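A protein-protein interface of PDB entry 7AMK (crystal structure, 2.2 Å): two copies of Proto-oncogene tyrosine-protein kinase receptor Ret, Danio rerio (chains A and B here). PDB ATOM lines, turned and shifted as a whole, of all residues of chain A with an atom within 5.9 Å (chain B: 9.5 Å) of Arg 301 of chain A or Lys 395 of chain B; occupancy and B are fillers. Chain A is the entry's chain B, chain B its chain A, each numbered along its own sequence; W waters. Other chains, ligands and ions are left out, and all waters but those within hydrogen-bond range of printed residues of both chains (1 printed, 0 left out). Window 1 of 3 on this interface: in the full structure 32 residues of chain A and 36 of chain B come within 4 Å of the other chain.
The side-chain amino group (NZ) of Lys 395 of chain B is in salt-bridge range of the side-chain carboxylate (OE2) of Glu 303 of chain A.
OE1 of Gln 394 of chain B lies within hydrogen-bond range of N of Glu 302 of chain A (3.3 Å).
NH1 of Arg 301 of chain A is in salt-bridge range of OE2 of Glu 316 of chain A (2.8 Å).
The backbone NH (N) of Gly 312 of chain A sits at hydrogen-bond distance from the backbone carbonyl oxygen (O) of Glu 303 of chain A, at 2.7 Å.
The side-chain carboxylate of Glu 303 of chain A is in salt-bridge range of the guanidinium group of Arg 301 of chain A, 2.5 Å away.
NE2 of Gln 394 of chain B is in hydrogen-bond range of SG of Cys 389 of chain B.
The backbone carbonyl oxygen (O) of Arg 301 of chain A lies within hydrogen-bond range of the backbone NH (N) of Val 314 of chain A (2.9 Å).
The side-chain sulfur of Cys 393 of chain B is disulfide-bonded to the side-chain sulfur of Cys 389 of chain B (2.0 Å).
Gln 394 of chain B touches Arg 301 of chain A (OE1 to CA, 3.4 Å).
Arg 301 of chain A touches Lys 395 of chain B (NH2 to NZ, 3.6 Å).
OD1 of Asn 392 of chain B touches CG of Glu 303 of chain A, at 3.6 Å.
OD1 of Asn 392 of chain B touches N of Ala 305 of chain A, at 3.6 Å.
Of chain B, only Gln 394 (3.4 Å) and Lys 395 (3.6 Å) come within 4 Å of Arg 301 of chain A.
Of the printed residues of chain B, Glu 302 of chain A touches Gln 394.
Printed residues of chain B within 4 Å of Glu 303 of chain A: Asn 392 (3.6 Å) and Lys 395 (2.7 Å).
No residue of chain B comes within 4 Å of Val 314 of chain A.
Leu 245 of chain B touches none of the printed residues of chain A.
Of chain A, only Arg 301 (3.6 Å) and Glu 303 (2.7 Å) come within 4 Å of Lys 395 of chain B.
The nearest residue of chain B that does not touch Arg 301 of chain A is Asn 392 of chain B (6.8 Å).
Of the 12 printed residues of chain A, 4 touch a printed residue of chain B.
Printed residues of chain A that touch a printed residue of chain B: Arg 301, Glu 302, Glu 303 and Ala 305.
Printed residues of chain B that touch a printed residue of chain A: Asn 392, Gln 394 and Lys 395.
Among the printed residues, Asp or Glu carboxylates within 4 Å of a Lys or Arg side-chain nitrogen of the other chain: Glu 303 of chain A with Lys 395 of chain B.
No position is printed for both chains.
Of the 6 pairs that touch across the chains among the printed residues, none has its exchanged pair printed and touching as well.
Water W1 lies within hydrogen-bond range of O of Glu 302 of chain A, NE2 of Gln 394 of chain B and SG of Cys 389 of chain B.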
ATOM      1  N   PHE A 260     -34.815 -24.216 -15.782  1.00  0.00           N
ATOM      2  CA  PHE A 260     -33.899 -24.072 -14.653  1.00  0.00           C
ATOM      3  C   PHE A 260     -33.868 -25.363 -13.838  1.00  0.00           C
ATOM      4  O   PHE A 260     -34.913 -25.844 -13.384  1.00  0.00           O
ATOM      5  CB  PHE A 260     -34.292 -22.881 -13.772  1.00  0.00           C
ATOM      6  CG  PHE A 260     -34.204 -21.552 -14.480  1.00  0.00           C
ATOM      7  CD1 PHE A 260     -32.968 -20.980 -14.753  1.00  0.00           C
ATOM      8  CD2 PHE A 260     -35.353 -20.894 -14.907  1.00  0.00           C
ATOM      9  CE1 PHE A 260     -32.876 -19.772 -15.424  1.00  0.00           C
ATOM     10  CE2 PHE A 260     -35.265 -19.679 -15.578  1.00  0.00           C
ATOM     11  CZ  PHE A 260     -34.030 -19.120 -15.832  1.00  0.00           C
ATOM     12  N   LYS A 299     -25.538 -24.516 -19.747  1.00  0.00           N
ATOM     13  CA  LYS A 299     -24.570 -23.743 -18.988  1.00  0.00           C
ATOM     14  C   LYS A 299     -24.947 -23.837 -17.519  1.00  0.00           C
ATOM     15  O   LYS A 299     -26.084 -24.178 -17.167  1.00  0.00           O
ATOM     16  CB  LYS A 299     -24.498 -22.273 -19.456  1.00  0.00           C
ATOM     17  CG  LYS A 299     -25.808 -21.672 -19.949  1.00  0.00           C
ATOM     18  N   PHE A 300     -23.973 -23.562 -16.655  1.00  0.00           N
ATOM     19  CA  PHE A 300     -24.225 -23.609 -15.225  1.00  0.00           C
ATOM     20  C   PHE A 300     -23.246 -22.706 -14.498  1.00  0.00           C
ATOM     21  O   PHE A 300     -22.188 -22.340 -15.016  1.00  0.00           O
ATOM     22  CB  PHE A 300     -24.131 -25.035 -14.665  1.00  0.00           C
ATOM     23  CG  PHE A 300     -22.721 -25.541 -14.500  1.00  0.00           C
ATOM     24  CD1 PHE A 300     -22.076 -26.189 -15.544  1.00  0.00           C
ATOM     25  CD2 PHE A 300     -22.046 -25.381 -13.296  1.00  0.00           C
ATOM     26  CE1 PHE A 300     -20.788 -26.666 -15.395  1.00  0.00           C
ATOM     27  CE2 PHE A 300     -20.755 -25.854 -13.143  1.00  0.00           C
ATOM     28  CZ  PHE A 300     -20.130 -26.505 -14.201  1.00  0.00           C
ATOM     29  N   ARG A 301     -23.622 -22.362 -13.272  1.00  0.00           N
ATOM     30  CA  ARG A 301     -22.837 -21.481 -12.432  1.00  0.00           C
ATOM     31  C   ARG A 301     -23.108 -21.867 -10.993  1.00  0.00           C
ATOM     32  O   ARG A 301     -24.118 -22.506 -10.677  1.00  0.00           O
ATOM     33  CB  ARG A 301     -23.195 -20.006 -12.667  1.00  0.00           C
ATOM     34  CG  ARG A 301     -24.621 -19.666 -12.230  1.00  0.00           C
ATOM     35  CD  ARG A 301     -24.960 -18.202 -12.470  1.00  0.00           C
ATOM     36  NE  ARG A 301     -26.316 -17.899 -12.030  1.00  0.00           N
ATOM     37  CZ  ARG A 301     -27.401 -18.058 -12.781  1.00  0.00           C
ATOM     38  NH1 ARG A 301     -27.324 -18.516 -14.018  1.00  0.00           N
ATOM     39  NH2 ARG A 301     -28.594 -17.747 -12.278  1.00  0.00           N
ATOM     40  N   GLU A 302     -22.195 -21.475 -10.118  1.00  0.00           N
ATOM     41  CA  GLU A 302     -22.423 -21.663  -8.697  1.00  0.00           C
ATOM     42  C   GLU A 302     -22.970 -20.365  -8.121  1.00  0.00           C
ATOM     43  O   GLU A 302     -22.691 -19.277  -8.623  1.00  0.00           O
ATOM     44  CB  GLU A 302     -21.149 -22.104  -7.975  1.00  0.00           C
ATOM     45  CG  GLU A 302     -20.604 -23.462  -8.438  1.00  0.00           C
ATOM     46  CD  GLU A 302     -19.857 -24.199  -7.327  1.00  0.00           C
ATOM     47  OE1 GLU A 302     -20.227 -24.015  -6.145  1.00  0.00           O
ATOM     48  OE2 GLU A 302     -18.911 -24.963  -7.625  1.00  0.00           O
ATOM     49  N   GLU A 303     -23.777 -20.491  -7.076  1.00  0.00           N
ATOM     50  CA  GLU A 303     -24.563 -19.360  -6.618  1.00  0.00           C
ATOM     51  C   GLU A 303     -24.962 -19.571  -5.169  1.00  0.00           C
ATOM     52  O   GLU A 303     -25.394 -20.657  -4.786  1.00  0.00           O
ATOM     53  CB  GLU A 303     -25.817 -19.179  -7.476  1.00  0.00           C
ATOM     54  CG  GLU A 303     -26.050 -17.750  -7.874  1.00  0.00           C
ATOM     55  CD  GLU A 303     -27.380 -17.557  -8.546  1.00  0.00           C
ATOM     56  OE1 GLU A 303     -28.403 -17.492  -7.828  1.00  0.00           O
ATOM     57  OE2 GLU A 303     -27.402 -17.473  -9.792  1.00  0.00           O
ATOM     58  N   ALA A 305     -26.869 -16.782  -3.816  1.00  0.00           N
ATOM     59  CA  ALA A 305     -27.990 -15.854  -3.700  1.00  0.00           C
ATOM     60  C   ALA A 305     -29.329 -16.583  -3.777  1.00  0.00           C
ATOM     61  O   ALA A 305     -30.178 -16.439  -2.889  1.00  0.00           O
ATOM     62  CB  ALA A 305     -27.883 -14.780  -4.787  1.00  0.00           C
ATOM     63  N   GLY A 312     -24.837 -23.047  -3.782  1.00  0.00           N
ATOM     64  CA  GLY A 312     -25.359 -24.177  -4.524  1.00  0.00           C
ATOM     65  C   GLY A 312     -25.065 -24.039  -6.002  1.00  0.00           C
ATOM     66  O   GLY A 312     -24.275 -23.176  -6.399  1.00  0.00           O
ATOM     67  N   THR A 313     -25.691 -24.863  -6.833  1.00  0.00           N
ATOM     68  CA  THR A 313     -25.395 -24.893  -8.256  1.00  0.00           C
ATOM     69  C   THR A 313     -26.677 -24.630  -9.030  1.00  0.00           C
ATOM     70  O   THR A 313     -27.706 -25.269  -8.771  1.00  0.00           O
ATOM     71  CB  THR A 313     -24.783 -26.239  -8.683  1.00  0.00           C
ATOM     72  OG1 THR A 313     -23.684 -26.591  -7.824  1.00  0.00           O
ATOM     73  CG2 THR A 313     -24.263 -26.141 -10.104  1.00  0.00           C
ATOM     74  N   VAL A 314     -26.621 -23.685  -9.962  1.00  0.00           N
ATOM     75  CA  VAL A 314     -27.735 -23.369 -10.848  1.00  0.00           C
ATOM     76  C   VAL A 314     -27.349 -23.763 -12.268  1.00  0.00           C
ATOM     77  O   VAL A 314     -26.298 -23.342 -12.773  1.00  0.00           O
ATOM     78  CB  VAL A 314     -28.123 -21.881 -10.790  1.00  0.00           C
ATOM     79  CG1 VAL A 314     -29.170 -21.594 -11.848  1.00  0.00           C
ATOM     80  CG2 VAL A 314     -28.687 -21.531  -9.444  1.00  0.00           C
ATOM     81  N   HIS A 315     -28.204 -24.555 -12.911  1.00  0.00           N
ATOM     82  CA  HIS A 315     -28.014 -25.001 -14.285  1.00  0.00           C
ATOM     83  C   HIS A 315     -29.092 -24.416 -15.179  1.00  0.00           C
ATOM     84  O   HIS A 315     -30.276 -24.433 -14.828  1.00  0.00           O
ATOM     85  CB  HIS A 315     -28.089 -26.520 -14.396  1.00  0.00           C
ATOM     86  CG  HIS A 315     -27.075 -27.240 -13.574  1.00  0.00           C
ATOM     87  ND1 HIS A 315     -26.036 -27.947 -14.137  1.00  0.00           N
ATOM     88  CD2 HIS A 315     -26.956 -27.394 -12.236  1.00  0.00           C
ATOM     89  CE1 HIS A 315     -25.311 -28.495 -13.179  1.00  0.00           C
ATOM     90  NE2 HIS A 315     -25.849 -28.179 -12.017  1.00  0.00           N
ATOM     91  N   GLU A 316     -28.687 -23.966 -16.359  1.00  0.00           N
ATOM     92  CA  GLU A 316     -29.611 -23.430 -17.347  1.00  0.00           C
ATOM     93  C   GLU A 316     -29.568 -24.295 -18.594  1.00  0.00           C
ATOM     94  O   GLU A 316     -28.486 -24.610 -19.094  1.00  0.00           O
ATOM     95  CB  GLU A 316     -29.269 -21.982 -17.690  1.00  0.00           C
ATOM     96  CG  GLU A 316     -29.504 -21.054 -16.534  1.00  0.00           C
ATOM     97  CD  GLU A 316     -29.195 -19.639 -16.886  1.00  0.00           C
ATOM     98  OE1 GLU A 316     -28.820 -19.398 -18.053  1.00  0.00           O
ATOM     99  OE2 GLU A 316     -29.323 -18.771 -16.002  1.00  0.00           O
ATOM    100  N   LEU B 245     -34.674  -3.894 -12.038  1.00  0.00           N
ATOM    101  CA  LEU B 245     -33.672  -4.156 -11.016  1.00  0.00           C
ATOM    102  C   LEU B 245     -32.306  -4.132 -11.676  1.00  0.00           C
ATOM    103  O   LEU B 245     -32.088  -4.821 -12.677  1.00  0.00           O
ATOM    104  CB  LEU B 245     -33.909  -5.503 -10.322  1.00  0.00           C
ATOM    105  CG  LEU B 245     -32.899  -5.838  -9.204  1.00  0.00           C
ATOM    106  CD1 LEU B 245     -32.971  -4.826  -8.065  1.00  0.00           C
ATOM    107  CD2 LEU B 245     -33.022  -7.268  -8.661  1.00  0.00           C
ATOM    108  N   GLU B 247     -28.550  -5.002 -10.555  1.00  0.00           N
ATOM    109  CA  GLU B 247     -27.776  -5.649  -9.507  1.00  0.00           C
ATOM    110  C   GLU B 247     -26.503  -6.227 -10.109  1.00  0.00           C
ATOM    111  O   GLU B 247     -25.566  -5.476 -10.405  1.00  0.00           O
ATOM    112  CB  GLU B 247     -28.613  -6.729  -8.805  1.00  0.00           C
ATOM    113  CG  GLU B 247     -27.910  -7.363  -7.576  1.00  0.00           C
ATOM    114  CD  GLU B 247     -28.858  -8.146  -6.668  1.00  0.00           C
ATOM    115  OE1 GLU B 247     -29.988  -8.473  -7.100  1.00  0.00           O
ATOM    116  OE2 GLU B 247     -28.472  -8.432  -5.516  1.00  0.00           O
ATOM    117  N   PHE B 248     -26.475  -7.550 -10.314  1.00  0.00           N
ATOM    118  CA  PHE B 248     -25.251  -8.220 -10.748  1.00  0.00           C
ATOM    119  C   PHE B 248     -24.900  -7.926 -12.197  1.00  0.00           C
ATOM    120  O   PHE B 248     -23.744  -8.103 -12.582  1.00  0.00           O
ATOM    121  CB  PHE B 248     -25.378  -9.731 -10.530  1.00  0.00           C
ATOM    122  CG  PHE B 248     -25.571 -10.101  -9.095  1.00  0.00           C
ATOM    123  CD1 PHE B 248     -24.524  -9.998  -8.191  1.00  0.00           C
ATOM    124  CD2 PHE B 248     -26.802 -10.522  -8.634  1.00  0.00           C
ATOM    125  CE1 PHE B 248     -24.698 -10.322  -6.864  1.00  0.00           C
ATOM    126  CE2 PHE B 248     -26.980 -10.845  -7.304  1.00  0.00           C
ATOM    127  CZ  PHE B 248     -25.937 -10.743  -6.423  1.00  0.00           C
ATOM    128  N   ASP B 249     -25.855  -7.464 -13.002  1.00  0.00           N
ATOM    129  CA  ASP B 249     -25.592  -7.062 -14.381  1.00  0.00           C
ATOM    130  C   ASP B 249     -25.601  -5.546 -14.439  1.00  0.00           C
ATOM    131  O   ASP B 249     -26.664  -4.925 -14.371  1.00  0.00           O
ATOM    132  CB  ASP B 249     -26.625  -7.634 -15.349  1.00  0.00           C
ATOM    133  CG  ASP B 249     -26.383  -7.199 -16.796  1.00  0.00           C
ATOM    134  OD1 ASP B 249     -25.831  -6.098 -17.033  1.00  0.00           O
ATOM    135  OD2 ASP B 249     -26.747  -7.966 -17.712  1.00  0.00           O
ATOM    136  N   ARG B 250     -24.427  -4.961 -14.624  1.00  0.00           N
ATOM    137  CA  ARG B 250     -24.301  -3.515 -14.690  1.00  0.00           C
ATOM    138  C   ARG B 250     -23.552  -3.072 -15.941  1.00  0.00           C
ATOM    139  O   ARG B 250     -23.007  -1.971 -15.962  1.00  0.00           O
ATOM    140  CB  ARG B 250     -23.597  -2.997 -13.431  1.00  0.00           C
ATOM    141  CG  ARG B 250     -23.677  -3.948 -12.256  1.00  0.00           C
ATOM    142  CD  ARG B 250     -22.976  -3.388 -11.032  1.00  0.00           C
ATOM    143  NE  ARG B 250     -23.917  -2.968  -9.996  1.00  0.00           N
ATOM    144  CZ  ARG B 250     -24.134  -1.706  -9.653  1.00  0.00           C
ATOM    145  NH1 ARG B 250     -23.506  -0.718 -10.252  1.00  0.00           N
ATOM    146  NH2 ARG B 250     -24.996  -1.431  -8.679  1.00  0.00           N
ATOM    147  N   SER B 251     -23.496  -3.908 -16.979  1.00  0.00           N
ATOM    148  CA  SER B 251     -22.678  -3.598 -18.147  1.00  0.00           C
ATOM    149  C   SER B 251     -23.411  -2.642 -19.073  1.00  0.00           C
ATOM    150  O   SER B 251     -24.637  -2.701 -19.208  1.00  0.00           O
ATOM    151  CB  SER B 251     -22.290  -4.874 -18.908  1.00  0.00           C
ATOM    152  OG  SER B 251     -23.407  -5.650 -19.296  1.00  0.00           O
ATOM    153  N   PHE B 256     -32.640  -3.436 -19.615  1.00  0.00           N
ATOM    154  CA  PHE B 256     -33.185  -3.864 -18.335  1.00  0.00           C
ATOM    155  C   PHE B 256     -34.704  -3.858 -18.275  1.00  0.00           C
ATOM    156  O   PHE B 256     -35.264  -4.308 -17.270  1.00  0.00           O
ATOM    157  CB  PHE B 256     -32.630  -2.986 -17.203  1.00  0.00           C
ATOM    158  CG  PHE B 256     -31.182  -3.232 -16.913  1.00  0.00           C
ATOM    159  CD1 PHE B 256     -30.195  -2.587 -17.641  1.00  0.00           C
ATOM    160  CD2 PHE B 256     -30.806  -4.125 -15.932  1.00  0.00           C
ATOM    161  CE1 PHE B 256     -28.852  -2.821 -17.384  1.00  0.00           C
ATOM    162  CE2 PHE B 256     -29.474  -4.358 -15.667  1.00  0.00           C
ATOM    163  CZ  PHE B 256     -28.492  -3.702 -16.400  1.00  0.00           C
ATOM    164  N   VAL B 362     -23.460  -3.919  -5.134  1.00  0.00           N
ATOM    165  CA  VAL B 362     -22.920  -5.269  -5.240  1.00  0.00           C
ATOM    166  C   VAL B 362     -21.700  -5.363  -4.322  1.00  0.00           C
ATOM    167  O   VAL B 362     -20.663  -4.728  -4.593  1.00  0.00           O
ATOM    168  CB  VAL B 362     -22.579  -5.625  -6.691  1.00  0.00           C
ATOM    169  CG1 VAL B 362     -21.803  -6.916  -6.749  1.00  0.00           C
ATOM    170  CG2 VAL B 362     -23.890  -5.730  -7.502  1.00  0.00           C
ATOM    171  N   CYS B 389     -13.300 -17.143  -6.830  1.00  0.00           N
ATOM    172  CA  CYS B 389     -14.410 -16.302  -7.247  1.00  0.00           C
ATOM    173  C   CYS B 389     -14.996 -15.599  -6.024  1.00  0.00           C
ATOM    174  O   CYS B 389     -15.285 -16.248  -5.013  1.00  0.00           O
ATOM    175  CB  CYS B 389     -15.424 -17.197  -7.985  1.00  0.00           C
ATOM    176  SG  CYS B 389     -17.118 -16.636  -8.372  1.00  0.00           S
ATOM    177  N   VAL B 390     -15.142 -14.271  -6.084  1.00  0.00           N
ATOM    178  CA  VAL B 390     -15.840 -13.548  -5.019  1.00  0.00           C
ATOM    179  C   VAL B 390     -17.316 -13.940  -5.040  1.00  0.00           C
ATOM    180  O   VAL B 390     -17.782 -14.586  -5.980  1.00  0.00           O
ATOM    181  CB  VAL B 390     -15.684 -12.018  -5.160  1.00  0.00           C
ATOM    182  CG1 VAL B 390     -14.281 -11.573  -4.752  1.00  0.00           C
ATOM    183  CG2 VAL B 390     -16.014 -11.585  -6.590  1.00  0.00           C
ATOM    184  N   GLU B 391     -18.067 -13.544  -4.020  1.00  0.00           N
ATOM    185  CA  GLU B 391     -19.463 -13.958  -3.925  1.00  0.00           C
ATOM    186  C   GLU B 391     -20.245 -13.534  -5.169  1.00  0.00           C
ATOM    187  O   GLU B 391     -20.194 -12.376  -5.598  1.00  0.00           O
ATOM    188  CB  GLU B 391     -20.095 -13.377  -2.658  1.00  0.00           C
ATOM    189  CG  GLU B 391     -21.542 -13.812  -2.408  1.00  0.00           C
ATOM    190  CD  GLU B 391     -22.150 -13.117  -1.198  1.00  0.00           C
ATOM    191  OE1 GLU B 391     -21.592 -13.261  -0.089  1.00  0.00           O
ATOM    192  OE2 GLU B 391     -23.168 -12.412  -1.359  1.00  0.00           O
ATOM    193  N   ASN B 392     -20.943 -14.499  -5.768  1.00  0.00           N
ATOM    194  CA  ASN B 392     -21.809 -14.303  -6.935  1.00  0.00           C
ATOM    195  C   ASN B 392     -21.064 -13.751  -8.144  1.00  0.00           C
ATOM    196  O   ASN B 392     -21.697 -13.270  -9.092  1.00  0.00           O
ATOM    197  CB  ASN B 392     -23.007 -13.403  -6.605  1.00  0.00           C
ATOM    198  CG  ASN B 392     -24.029 -14.098  -5.724  1.00  0.00           C
ATOM    199  OD1 ASN B 392     -24.348 -15.270  -5.923  1.00  0.00           O
ATOM    200  ND2 ASN B 392     -24.539 -13.380  -4.738  1.00  0.00           N
ATOM    201  N   CYS B 393     -19.730 -13.848  -8.138  1.00  0.00           N
ATOM    202  CA  CYS B 393     -18.936 -13.351  -9.258  1.00  0.00           C
ATOM    203  C   CYS B 393     -19.402 -13.918 -10.596  1.00  0.00           C
ATOM    204  O   CYS B 393     -19.241 -13.260 -11.628  1.00  0.00           O
ATOM    205  CB  CYS B 393     -17.457 -13.679  -9.044  1.00  0.00           C
ATOM    206  SG  CYS B 393     -16.950 -15.226  -9.845  1.00  0.00           S
ATOM    207  N   GLN B 394     -19.974 -15.130 -10.612  1.00  0.00           N
ATOM    208  CA  GLN B 394     -20.337 -15.742 -11.888  1.00  0.00           C
ATOM    209  C   GLN B 394     -21.584 -15.126 -12.505  1.00  0.00           C
ATOM    210  O   GLN B 394     -21.832 -15.338 -13.695  1.00  0.00           O
ATOM    211  CB  GLN B 394     -20.518 -17.258 -11.733  1.00  0.00           C
ATOM    212  CG  GLN B 394     -19.199 -18.023 -11.771  1.00  0.00           C
ATOM    213  CD  GLN B 394     -19.292 -19.410 -11.167  1.00  0.00           C
ATOM    214  OE1 GLN B 394     -19.631 -20.368 -11.844  1.00  0.00           O
ATOM    215  NE2 GLN B 394     -18.981 -19.519  -9.881  1.00  0.00           N
ATOM    216  N   LYS B 395     -22.354 -14.362 -11.733  1.00  0.00           N
ATOM    217  CA  LYS B 395     -23.457 -13.555 -12.243  1.00  0.00           C
ATOM    218  C   LYS B 395     -23.008 -12.174 -12.717  1.00  0.00           C
ATOM    219  O   LYS B 395     -23.833 -11.428 -13.242  1.00  0.00           O
ATOM    220  CB  LYS B 395     -24.532 -13.379 -11.155  1.00  0.00           C
ATOM    221  CG  LYS B 395     -24.950 -14.656 -10.422  1.00  0.00           C
ATOM    222  CD  LYS B 395     -25.776 -14.357  -9.158  1.00  0.00           C
ATOM    223  CE  LYS B 395     -27.167 -13.850  -9.484  1.00  0.00           C
ATOM    224  NZ  LYS B 395     -28.033 -14.901 -10.112  1.00  0.00           N
ATOM    225  N   PHE B 396     -21.737 -11.808 -12.526  1.00  0.00           N
ATOM    226  CA  PHE B 396     -21.300 -10.443 -12.801  1.00  0.00           C
ATOM    227  C   PHE B 396     -21.241 -10.170 -14.295  1.00  0.00           C
ATOM    228  O   PHE B 396     -20.811 -11.014 -15.078  1.00  0.00           O
ATOM    229  CB  PHE B 396     -19.919 -10.172 -12.197  1.00  0.00           C
ATOM    230  CG  PHE B 396     -19.921 -10.020 -10.700  1.00  0.00           C
ATOM    231  CD1 PHE B 396     -21.104 -10.085  -9.983  1.00  0.00           C
ATOM    232  CD2 PHE B 396     -18.741  -9.806 -10.009  1.00  0.00           C
ATOM    233  CE1 PHE B 396     -21.108  -9.951  -8.616  1.00  0.00           C
ATOM    234  CE2 PHE B 396     -18.744  -9.671  -8.638  1.00  0.00           C
ATOM    235  CZ  PHE B 396     -19.918  -9.743  -7.941  1.00  0.00           C
ATOM    236  N   LYS B 397     -21.642  -8.959 -14.673  1.00  0.00           N
ATOM    237  CA  LYS B 397     -21.516  -8.454 -16.036  1.00  0.00           C
ATOM    238  C   LYS B 397     -21.304  -6.948 -15.941  1.00  0.00           C
ATOM    239  O   LYS B 397     -22.118  -6.244 -15.332  1.00  0.00           O
ATOM    240  CB  LYS B 397     -22.759  -8.786 -16.875  1.00  0.00           C
ATOM    241  N   GLY B 398     -20.222  -6.449 -16.538  1.00  0.00           N
ATOM    242  CA  GLY B 398     -19.857  -5.056 -16.373  1.00  0.00           C
ATOM    243  C   GLY B 398     -19.068  -4.748 -15.118  1.00  0.00           C
ATOM    244  O   GLY B 398     -18.853  -3.569 -14.805  1.00  0.00           O
ATOM    245  N   ILE B 399     -18.631  -5.773 -14.390  1.00  0.00           N
ATOM    246  CA  ILE B 399     -17.854  -5.631 -13.163  1.00  0.00           C
ATOM    247  C   ILE B 399     -16.550  -6.377 -13.376  1.00  0.00           C
ATOM    248  O   ILE B 399     -16.555  -7.601 -13.549  1.00  0.00           O
ATOM    249  CB  ILE B 399     -18.601  -6.196 -11.941  1.00  0.00           C
ATOM    250  CG1 ILE B 399     -20.002  -5.577 -11.832  1.00  0.00           C
ATOM    251  CG2 ILE B 399     -17.782  -5.995 -10.687  1.00  0.00           C
ATOM    252  CD1 ILE B 399     -20.923  -6.287 -10.869  1.00  0.00           C
ATOM    253  N   TYR B 403      -7.769 -11.170  -9.868  1.00  0.00           N
ATOM    254  CA  TYR B 403      -7.356 -12.000  -8.746  1.00  0.00           C
ATOM    255  C   TYR B 403      -5.838 -12.142  -8.724  1.00  0.00           C
ATOM    256  O   TYR B 403      -5.187 -12.185  -9.772  1.00  0.00           O
ATOM    257  CB  TYR B 403      -8.021 -13.379  -8.823  1.00  0.00           C
ATOM    258  CG  TYR B 403      -9.536 -13.327  -8.768  1.00  0.00           C
ATOM    259  CD1 TYR B 403     -10.286 -13.090  -9.909  1.00  0.00           C
ATOM    260  CD2 TYR B 403     -10.215 -13.485  -7.561  1.00  0.00           C
ATOM    261  CE1 TYR B 403     -11.673 -13.024  -9.862  1.00  0.00           C
ATOM    262  CE2 TYR B 403     -11.610 -13.412  -7.502  1.00  0.00           C
ATOM    263  CZ  TYR B 403     -12.329 -13.186  -8.653  1.00  0.00           C
ATOM    264  OH  TYR B 403     -13.703 -13.120  -8.598  1.00  0.00           O
ATOM    265  N   ASN B 430     -13.876 -14.464 -18.746  1.00  0.00           N
ATOM    266  CA  ASN B 430     -15.171 -15.016 -19.140  1.00  0.00           C
ATOM    267  C   ASN B 430     -16.185 -14.910 -18.004  1.00  0.00           C
ATOM    268  O   ASN B 430     -17.350 -14.555 -18.231  1.00  0.00           O
ATOM    269  CB  ASN B 430     -15.019 -16.475 -19.580  1.00  0.00           C
ATOM    270  CG  ASN B 430     -14.313 -16.612 -20.912  1.00  0.00           C
ATOM    271  OD1 ASN B 430     -13.691 -15.667 -21.400  1.00  0.00           O
ATOM    272  ND2 ASN B 430     -14.402 -17.794 -21.510  1.00  0.00           N
ATOM    273  N   ASP B 431     -15.753 -15.216 -16.771  1.00  0.00           N
ATOM    274  CA  ASP B 431     -16.608 -15.176 -15.592  1.00  0.00           C
ATOM    275  C   ASP B 431     -16.222 -14.096 -14.599  1.00  0.00           C
ATOM    276  O   ASP B 431     -16.984 -13.846 -13.658  1.00  0.00           O
ATOM    277  CB  ASP B 431     -16.575 -16.521 -14.851  1.00  0.00           C
ATOM    278  CG  ASP B 431     -16.734 -17.694 -15.778  1.00  0.00           C
ATOM    279  OD1 ASP B 431     -17.544 -17.596 -16.726  1.00  0.00           O
ATOM    280  OD2 ASP B 431     -16.042 -18.712 -15.559  1.00  0.00           O
ATOM    281  N   ASN B 432     -15.076 -13.449 -14.780  1.00  0.00           N
ATOM    282  CA  ASN B 432     -14.426 -12.740 -13.683  1.00  0.00           C
ATOM    283  C   ASN B 432     -14.044 -13.738 -12.590  1.00  0.00           C
ATOM    284  O   ASN B 432     -14.165 -13.470 -11.394  1.00  0.00           O
ATOM    285  CB  ASN B 432     -15.315 -11.618 -13.136  1.00  0.00           C
ATOM    286  N   THR B 433     -13.611 -14.920 -13.020  1.00  0.00           N
ATOM    287  CA  THR B 433     -13.177 -16.006 -12.157  1.00  0.00           C
ATOM    288  C   THR B 433     -11.654 -16.111 -12.199  1.00  0.00           C
ATOM    289  O   THR B 433     -10.998 -15.626 -13.126  1.00  0.00           O
ATOM    290  CB  THR B 433     -13.842 -17.322 -12.596  1.00  0.00           C
ATOM    291  OG1 THR B 433     -13.383 -18.419 -11.801  1.00  0.00           O
ATOM    292  CG2 THR B 433     -13.530 -17.617 -14.035  1.00  0.00           C
HETATM  293  O   HOH W   1     -20.703 -17.513  -8.356  1.00  0.00           O
